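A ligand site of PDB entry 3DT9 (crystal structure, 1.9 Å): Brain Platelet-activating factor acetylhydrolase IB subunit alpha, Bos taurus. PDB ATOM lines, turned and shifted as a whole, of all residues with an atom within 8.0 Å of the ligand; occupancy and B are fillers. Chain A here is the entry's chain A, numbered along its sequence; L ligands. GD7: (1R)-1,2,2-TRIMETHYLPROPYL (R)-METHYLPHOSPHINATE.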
ATOM      1  N   ARG A  22      22.708 -41.086  39.564  1.00  0.00           N
ATOM      2  CA  ARG A  22      21.996 -40.480  38.426  1.00  0.00           C
ATOM      3  C   ARG A  22      22.702 -40.588  37.078  1.00  0.00           C
ATOM      4  O   ARG A  22      22.033 -40.811  36.049  1.00  0.00           O
ATOM      5  CB  ARG A  22      21.639 -39.007  38.713  1.00  0.00           C
ATOM      6  CG  ARG A  22      20.614 -38.861  39.830  1.00  0.00           C
ATOM      7  CD  ARG A  22      20.167 -37.423  39.980  1.00  0.00           C
ATOM      8  NE  ARG A  22      21.270 -36.491  40.049  1.00  0.00           N
ATOM      9  CZ  ARG A  22      21.606 -35.603  39.107  1.00  0.00           C
ATOM     10  NH1 ARG A  22      20.903 -35.481  37.995  1.00  0.00           N
ATOM     11  NH2 ARG A  22      22.652 -34.828  39.309  1.00  0.00           N
ATOM     12  N   GLY A  45      25.936 -35.189  24.120  1.00  0.00           N
ATOM     13  CA  GLY A  45      26.754 -34.123  24.632  1.00  0.00           C
ATOM     14  C   GLY A  45      26.374 -33.762  26.041  1.00  0.00           C
ATOM     15  O   GLY A  45      25.933 -34.588  26.818  1.00  0.00           O
ATOM     16  N   ASP A  46      26.511 -32.479  26.338  1.00  0.00           N
ATOM     17  CA  ASP A  46      26.287 -32.032  27.690  1.00  0.00           C
ATOM     18  C   ASP A  46      24.873 -31.452  27.907  1.00  0.00           C
ATOM     19  O   ASP A  46      23.906 -31.719  27.159  1.00  0.00           O
ATOM     20  CB  ASP A  46      27.378 -31.023  28.145  1.00  0.00           C
ATOM     21  CG  ASP A  46      27.468 -29.798  27.227  1.00  0.00           C
ATOM     22  OD1 ASP A  46      26.442 -29.420  26.602  1.00  0.00           O
ATOM     23  OD2 ASP A  46      28.564 -29.199  27.128  1.00  0.00           O
ATOM     24  N   SER A  47      24.674 -30.506  28.985  1.00  0.00           N
ATOM     25  CA  SER A  47      23.378 -29.929  29.343  1.00  0.00           C
ATOM     26  C   SER A  47      22.763 -29.182  28.188  1.00  0.00           C
ATOM     27  O   SER A  47      21.544 -29.217  27.976  1.00  0.00           O
ATOM     28  CB  SER A  47      23.571 -28.982  30.498  1.00  0.00           C
ATOM     29  OG  SER A  47      24.432 -27.892  30.133  1.00  0.00           O
ATOM     30  N   LEU A  48      23.637 -28.566  27.246  1.00  0.00           N
ATOM     31  CA  LEU A  48      23.089 -27.804  26.077  1.00  0.00           C
ATOM     32  C   LEU A  48      22.351 -28.718  25.132  1.00  0.00           C
ATOM     33  O   LEU A  48      21.364 -28.317  24.522  1.00  0.00           O
ATOM     34  CB  LEU A  48      24.210 -27.034  25.405  1.00  0.00           C
ATOM     35  CG  LEU A  48      24.714 -25.891  26.299  1.00  0.00           C
ATOM     36  CD1 LEU A  48      26.090 -25.493  25.835  1.00  0.00           C
ATOM     37  CD2 LEU A  48      23.795 -24.678  26.173  1.00  0.00           C
ATOM     38  N   VAL A  49      22.829 -29.957  25.009  1.00  0.00           N
ATOM     39  CA  VAL A  49      22.152 -30.953  24.182  1.00  0.00           C
ATOM     40  C   VAL A  49      20.935 -31.463  24.902  1.00  0.00           C
ATOM     41  O   VAL A  49      19.843 -31.509  24.328  1.00  0.00           O
ATOM     42  CB  VAL A  49      23.103 -32.188  23.871  1.00  0.00           C
ATOM     43  CG1 VAL A  49      22.295 -33.360  23.320  1.00  0.00           C
ATOM     44  CG2 VAL A  49      24.179 -31.774  22.956  1.00  0.00           C
ATOM     45  N   GLN A  50      21.103 -31.874  26.162  1.00  0.00           N
ATOM     46  CA  GLN A  50      20.032 -32.448  26.953  1.00  0.00           C
ATOM     47  C   GLN A  50      18.787 -31.543  26.993  1.00  0.00           C
ATOM     48  O   GLN A  50      17.686 -32.000  26.683  1.00  0.00           O
ATOM     49  CB  GLN A  50      20.553 -32.712  28.363  1.00  0.00           C
ATOM     50  CG  GLN A  50      19.573 -33.353  29.316  1.00  0.00           C
ATOM     51  CD  GLN A  50      20.167 -33.533  30.692  1.00  0.00           C
ATOM     52  OE1 GLN A  50      20.897 -32.653  31.176  1.00  0.00           O
ATOM     53  NE2 GLN A  50      19.893 -34.661  31.320  1.00  0.00           N
ATOM     54  N   LEU A  51      18.986 -30.263  27.336  1.00  0.00           N
ATOM     55  CA  LEU A  51      17.882 -29.305  27.509  1.00  0.00           C
ATOM     56  C   LEU A  51      17.228 -28.904  26.178  1.00  0.00           C
ATOM     57  O   LEU A  51      16.158 -28.290  26.157  1.00  0.00           O
ATOM     58  CB  LEU A  51      18.346 -28.065  28.274  1.00  0.00           C
ATOM     59  CG  LEU A  51      18.678 -28.417  29.724  1.00  0.00           C
ATOM     60  CD1 LEU A  51      19.255 -27.185  30.401  1.00  0.00           C
ATOM     61  CD2 LEU A  51      17.462 -28.927  30.444  1.00  0.00           C
ATOM     62  N   GLY A  71      22.000 -36.325  25.848  1.00  0.00           N
ATOM     63  CA  GLY A  71      22.727 -35.283  26.559  1.00  0.00           C
ATOM     64  C   GLY A  71      22.690 -35.566  28.041  1.00  0.00           C
ATOM     65  O   GLY A  71      21.676 -36.048  28.568  1.00  0.00           O
ATOM     66  N   ILE A  72      23.793 -35.252  28.717  1.00  0.00           N
ATOM     67  CA  ILE A  72      23.855 -35.385  30.158  1.00  0.00           C
ATOM     68  C   ILE A  72      24.495 -34.131  30.732  1.00  0.00           C
ATOM     69  O   ILE A  72      25.640 -33.758  30.351  1.00  0.00           O
ATOM     70  CB  ILE A  72      24.644 -36.628  30.620  1.00  0.00           C
ATOM     71  CG1 ILE A  72      23.957 -37.948  30.216  1.00  0.00           C
ATOM     72  CG2 ILE A  72      24.848 -36.576  32.161  1.00  0.00           C
ATOM     73  CD1 ILE A  72      24.706 -39.180  30.725  1.00  0.00           C
ATOM     74  N   GLY A  73      23.790 -33.461  31.642  1.00  0.00           N
ATOM     75  CA  GLY A  73      24.364 -32.272  32.271  1.00  0.00           C
ATOM     76  C   GLY A  73      25.696 -32.525  32.977  1.00  0.00           C
ATOM     77  O   GLY A  73      25.835 -33.513  33.696  1.00  0.00           O
ATOM     78  N   GLY A  74      26.688 -31.637  32.758  1.00  0.00           N
ATOM     79  CA  GLY A  74      27.980 -31.719  33.401  1.00  0.00           C
ATOM     80  C   GLY A  74      29.058 -32.513  32.672  1.00  0.00           C
ATOM     81  O   GLY A  74      30.221 -32.429  33.047  1.00  0.00           O
ATOM     82  N   ASP A  75      28.693 -33.242  31.614  1.00  0.00           N
ATOM     83  CA  ASP A  75      29.657 -34.091  30.897  1.00  0.00           C
ATOM     84  C   ASP A  75      30.750 -33.273  30.198  1.00  0.00           C
ATOM     85  O   ASP A  75      30.475 -32.229  29.585  1.00  0.00           O
ATOM     86  CB  ASP A  75      28.932 -34.980  29.842  1.00  0.00           C
ATOM     87  CG  ASP A  75      28.542 -36.300  30.378  1.00  0.00           C
ATOM     88  OD1 ASP A  75      28.522 -36.450  31.632  1.00  0.00           O
ATOM     89  OD2 ASP A  75      28.284 -37.200  29.553  1.00  0.00           O
ATOM     90  N   SER A  76      31.973 -33.788  30.292  1.00  0.00           N
ATOM     91  CA  SER A  76      33.128 -33.295  29.536  1.00  0.00           C
ATOM     92  C   SER A  76      33.336 -34.286  28.392  1.00  0.00           C
ATOM     93  O   SER A  76      32.638 -35.315  28.324  1.00  0.00           O
ATOM     94  CB  SER A  76      34.383 -33.247  30.422  1.00  0.00           C
ATOM     95  OG  SER A  76      34.259 -32.220  31.372  1.00  0.00           O
ATOM     96  N   TRP A 100      28.061 -32.243  20.792  1.00  0.00           N
ATOM     97  CA  TRP A 100      28.170 -30.903  21.377  1.00  0.00           C
ATOM     98  C   TRP A 100      28.637 -31.019  22.832  1.00  0.00           C
ATOM     99  O   TRP A 100      27.836 -31.283  23.722  1.00  0.00           O
ATOM    100  CB  TRP A 100      26.793 -30.226  21.352  1.00  0.00           C
ATOM    101  CG  TRP A 100      26.872 -28.739  21.484  1.00  0.00           C
ATOM    102  CD1 TRP A 100      28.000 -27.961  21.420  1.00  0.00           C
ATOM    103  CD2 TRP A 100      25.767 -27.845  21.605  1.00  0.00           C
ATOM    104  NE1 TRP A 100      27.650 -26.620  21.516  1.00  0.00           N
ATOM    105  CE2 TRP A 100      26.288 -26.528  21.630  1.00  0.00           C
ATOM    106  CE3 TRP A 100      24.376 -28.024  21.707  1.00  0.00           C
ATOM    107  CZ2 TRP A 100      25.466 -25.393  21.741  1.00  0.00           C
ATOM    108  CZ3 TRP A 100      23.560 -26.880  21.805  1.00  0.00           C
ATOM    109  CH2 TRP A 100      24.111 -25.591  21.833  1.00  0.00           C
ATOM    110  N   VAL A 101      29.926 -30.847  23.040  1.00  0.00           N
ATOM    111  CA  VAL A 101      30.546 -31.056  24.353  1.00  0.00           C
ATOM    112  C   VAL A 101      31.917 -30.354  24.350  1.00  0.00           C
ATOM    113  O   VAL A 101      32.544 -30.197  23.294  1.00  0.00           O
ATOM    114  CB  VAL A 101      30.684 -32.591  24.647  1.00  0.00           C
ATOM    115  CG1 VAL A 101      31.551 -33.274  23.575  1.00  0.00           C
ATOM    116  CG2 VAL A 101      31.262 -32.828  26.060  1.00  0.00           C
ATOM    117  N   GLY A 102      32.398 -29.937  25.518  1.00  0.00           N
ATOM    118  CA  GLY A 102      33.709 -29.330  25.655  1.00  0.00           C
ATOM    119  C   GLY A 102      33.669 -28.089  26.534  1.00  0.00           C
ATOM    120  O   GLY A 102      34.681 -27.726  27.116  1.00  0.00           O
ATOM    121  N   THR A 103      32.490 -27.474  26.691  1.00  0.00           N
ATOM    122  CA  THR A 103      32.376 -26.288  27.548  1.00  0.00           C
ATOM    123  C   THR A 103      32.607 -26.594  29.049  1.00  0.00           C
ATOM    124  O   THR A 103      32.943 -25.723  29.837  1.00  0.00           O
ATOM    125  CB  THR A 103      31.008 -25.547  27.352  1.00  0.00           C
ATOM    126  OG1 THR A 103      31.155 -24.182  27.710  1.00  0.00           O
ATOM    127  CG2 THR A 103      29.894 -26.201  28.207  1.00  0.00           C
ATOM    128  N   ASN A 104      32.434 -27.856  29.444  1.00  0.00           N
ATOM    129  CA  ASN A 104      32.621 -28.278  30.841  1.00  0.00           C
ATOM    130  C   ASN A 104      34.017 -28.806  31.171  1.00  0.00           C
ATOM    131  O   ASN A 104      34.268 -29.200  32.304  1.00  0.00           O
ATOM    132  CB  ASN A 104      31.604 -29.371  31.226  1.00  0.00           C
ATOM    133  CG  ASN A 104      30.163 -28.886  31.160  1.00  0.00           C
ATOM    134  OD1 ASN A 104      29.885 -27.711  31.405  1.00  0.00           O
ATOM    135  ND2 ASN A 104      29.225 -29.794  30.837  1.00  0.00           N
ATOM    136  N   HIS A 106      36.766 -28.076  32.351  1.00  0.00           N
ATOM    137  CA  HIS A 106      37.548 -27.186  33.200  1.00  0.00           C
ATOM    138  C   HIS A 106      38.853 -27.844  33.614  1.00  0.00           C
ATOM    139  O   HIS A 106      38.877 -29.008  34.057  1.00  0.00           O
ATOM    140  CB  HIS A 106      36.721 -26.755  34.408  1.00  0.00           C
ATOM    141  CG  HIS A 106      35.405 -26.167  34.005  1.00  0.00           C
ATOM    142  ND1 HIS A 106      35.313 -25.017  33.252  1.00  0.00           N
ATOM    143  CD2 HIS A 106      34.127 -26.607  34.190  1.00  0.00           C
ATOM    144  CE1 HIS A 106      34.027 -24.748  33.018  1.00  0.00           C
ATOM    145  NE2 HIS A 106      33.302 -25.700  33.574  1.00  0.00           N
ATOM    146  N   ARG A 141      30.157 -17.807  26.963  1.00  0.00           N
ATOM    147  CA  ARG A 141      29.489 -17.926  28.255  1.00  0.00           C
ATOM    148  C   ARG A 141      30.018 -16.799  29.157  1.00  0.00           C
ATOM    149  O   ARG A 141      31.065 -16.204  28.877  1.00  0.00           O
ATOM    150  CB  ARG A 141      29.764 -19.308  28.914  1.00  0.00           C
ATOM    151  CG  ARG A 141      31.242 -19.714  28.828  1.00  0.00           C
ATOM    152  CD  ARG A 141      31.441 -21.155  29.305  1.00  0.00           C
ATOM    153  NE  ARG A 141      31.225 -21.253  30.746  1.00  0.00           N
ATOM    154  CZ  ARG A 141      31.125 -22.400  31.435  1.00  0.00           C
ATOM    155  NH1 ARG A 141      31.233 -23.557  30.815  1.00  0.00           N
ATOM    156  NH2 ARG A 141      30.925 -22.383  32.752  1.00  0.00           N
ATOM    157  N   TYR A 191      19.869 -17.508  30.454  1.00  0.00           N
ATOM    158  CA  TYR A 191      19.356 -17.036  31.731  1.00  0.00           C
ATOM    159  C   TYR A 191      20.400 -17.002  32.850  1.00  0.00           C
ATOM    160  O   TYR A 191      20.286 -16.184  33.785  1.00  0.00           O
ATOM    161  CB  TYR A 191      18.102 -17.814  32.143  1.00  0.00           C
ATOM    162  CG  TYR A 191      18.270 -19.343  32.225  1.00  0.00           C
ATOM    163  CD1 TYR A 191      18.813 -19.940  33.355  1.00  0.00           C
ATOM    164  CD2 TYR A 191      17.885 -20.159  31.169  1.00  0.00           C
ATOM    165  CE1 TYR A 191      18.957 -21.340  33.440  1.00  0.00           C
ATOM    166  CE2 TYR A 191      18.037 -21.551  31.227  1.00  0.00           C
ATOM    167  CZ  TYR A 191      18.582 -22.128  32.371  1.00  0.00           C
ATOM    168  OH  TYR A 191      18.728 -23.497  32.446  1.00  0.00           O
ATOM    169  N   ASP A 192      21.401 -17.872  32.745  1.00  0.00           N
ATOM    170  CA  ASP A 192      22.505 -17.930  33.682  1.00  0.00           C
ATOM    171  C   ASP A 192      23.870 -17.743  32.971  1.00  0.00           C
ATOM    172  O   ASP A 192      24.905 -18.116  33.510  1.00  0.00           O
ATOM    173  CB  ASP A 192      22.459 -19.273  34.446  1.00  0.00           C
ATOM    174  CG  ASP A 192      22.763 -20.464  33.550  1.00  0.00           C
ATOM    175  OD1 ASP A 192      22.793 -20.294  32.326  1.00  0.00           O
ATOM    176  OD2 ASP A 192      22.982 -21.589  34.083  1.00  0.00           O
ATOM    177  N   LEU A 194      25.021 -19.288  30.528  1.00  0.00           N
ATOM    178  CA  LEU A 194      25.570 -20.586  30.069  1.00  0.00           C
ATOM    179  C   LEU A 194      24.504 -21.384  29.323  1.00  0.00           C
ATOM    180  O   LEU A 194      24.661 -21.686  28.116  1.00  0.00           O
ATOM    181  CB  LEU A 194      26.144 -21.415  31.251  1.00  0.00           C
ATOM    182  CG  LEU A 194      26.650 -22.843  30.896  1.00  0.00           C
ATOM    183  CD1 LEU A 194      27.729 -22.754  29.807  1.00  0.00           C
ATOM    184  CD2 LEU A 194      27.149 -23.548  32.179  1.00  0.00           C
ATOM    185  N   HIS A 195      23.440 -21.735  30.030  1.00  0.00           N
ATOM    186  CA  HIS A 195      22.320 -22.465  29.425  1.00  0.00           C
ATOM    187  C   HIS A 195      21.537 -21.514  28.559  1.00  0.00           C
ATOM    188  O   HIS A 195      21.496 -20.313  28.834  1.00  0.00           O
ATOM    189  CB  HIS A 195      21.360 -22.994  30.504  1.00  0.00           C
ATOM    190  CG  HIS A 195      21.953 -24.064  31.362  1.00  0.00           C
ATOM    191  ND1 HIS A 195      22.767 -23.791  32.452  1.00  0.00           N
ATOM    192  CD2 HIS A 195      21.839 -25.406  31.310  1.00  0.00           C
ATOM    193  CE1 HIS A 195      23.151 -24.924  33.005  1.00  0.00           C
ATOM    194  NE2 HIS A 195      22.577 -25.919  32.351  1.00  0.00           N
ATOM    195  N   LEU A 196      20.898 -22.043  27.516  1.00  0.00           N
ATOM    196  CA  LEU A 196      20.073 -21.238  26.602  1.00  0.00           C
ATOM    197  C   LEU A 196      18.609 -21.193  27.047  1.00  0.00           C
ATOM    198  O   LEU A 196      18.034 -22.195  27.455  1.00  0.00           O
ATOM    199  CB  LEU A 196      20.135 -21.843  25.187  1.00  0.00           C
ATOM    200  CG  LEU A 196      21.495 -21.685  24.499  1.00  0.00           C
ATOM    201  CD1 LEU A 196      21.619 -22.627  23.292  1.00  0.00           C
ATOM    202  CD2 LEU A 196      21.731 -20.232  24.088  1.00  0.00           C
HETATM  203  C1  GD7 L   1      24.932 -27.046  35.272  1.00  0.00           C
HETATM  204  C2  GD7 L   1      26.510 -28.887  35.755  1.00  0.00           C
HETATM  205  C3  GD7 L   1      24.451 -29.315  34.364  1.00  0.00           C
HETATM  206  C4  GD7 L   1      27.599 -27.113  33.714  1.00  0.00           C
HETATM  207  C5  GD7 L   1      26.358 -27.980  33.406  1.00  0.00           C
HETATM  208  C6  GD7 L   1      25.569 -28.307  34.664  1.00  0.00           C
HETATM  209  C7  GD7 L   1      26.806 -26.608  30.082  1.00  0.00           C
HETATM  210  OH  GD7 L   1      25.488 -27.413  32.400  1.00  0.00           O
HETATM  211  P1  GD7 L   1      25.818 -27.879  30.894  1.00  0.00           P
HETATM  212  O11 GD7 L   1      26.523 -29.293  30.866  1.00  0.00           O
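The backbone NH (N) of Ser 47 sits at hydrogen-bond distance from an oxygen (O11) of the ligand, 2.9 Å away. A phosphorus (P1) of the ligand is bonded to the side-chain hydroxyl of Ser 47 (1.6 Å). O11 of the ligand is in hydrogen-bond range of ND2 of Asn 104 (2.7 Å). N of Gly 74 sits at hydrogen-bond distance from O11 of the ligand. An oxygen (OH) of the ligand lies within hydrogen-bond range of a ring nitrogen (NE2) of His 195 (3.3 Å).
The side-chain amide nitrogen (ND2) of Asn 104 sits at hydrogen-bond distance from the backbone carbonyl oxygen (O) of Asp 75 (3.0 Å). The backbone carbonyl oxygen of Asn 104 sits at hydrogen-bond distance from the side-chain hydroxyl of Ser 76, 3.2 Å away. ND1 of His 195 sits at hydrogen-bond distance from OD2 of Asp 192, at 2.7 Å. The side-chain carboxylate of Asp 46 is in hydrogen-bond range of the backbone NH of Leu 48 (3.0 Å). N of Asp 46 lies within hydrogen-bond range of O of Trp 100. N of Gly 73 lies within hydrogen-bond range of OE1 of Gln 50, 3.0 Å away. The guanidinium group of Arg 141 is in hydrogen-bond range of the backbone carbonyl oxygen of Thr 103 (2.9 Å). N of Leu 194 lies within hydrogen-bond range of OD1 of Asp 192 (3.0 Å).
Asp 46 touches the ligand (CB to O11, 3.3 Å). Gly 73 touches the ligand (CA to C3, 3.6 Å). Thr 103 touches the ligand. CD2 of Leu 194 touches C7 of the ligand, 3.7 Å away. Hydrophobic or aromatic side chains that line the ligand: Leu 194 and His 195. Along chain A the residues within 4 Å of the ligand span positions 46 to 195. The nearest printed residue that does not touch the ligand is Leu 48 (4.3 Å).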
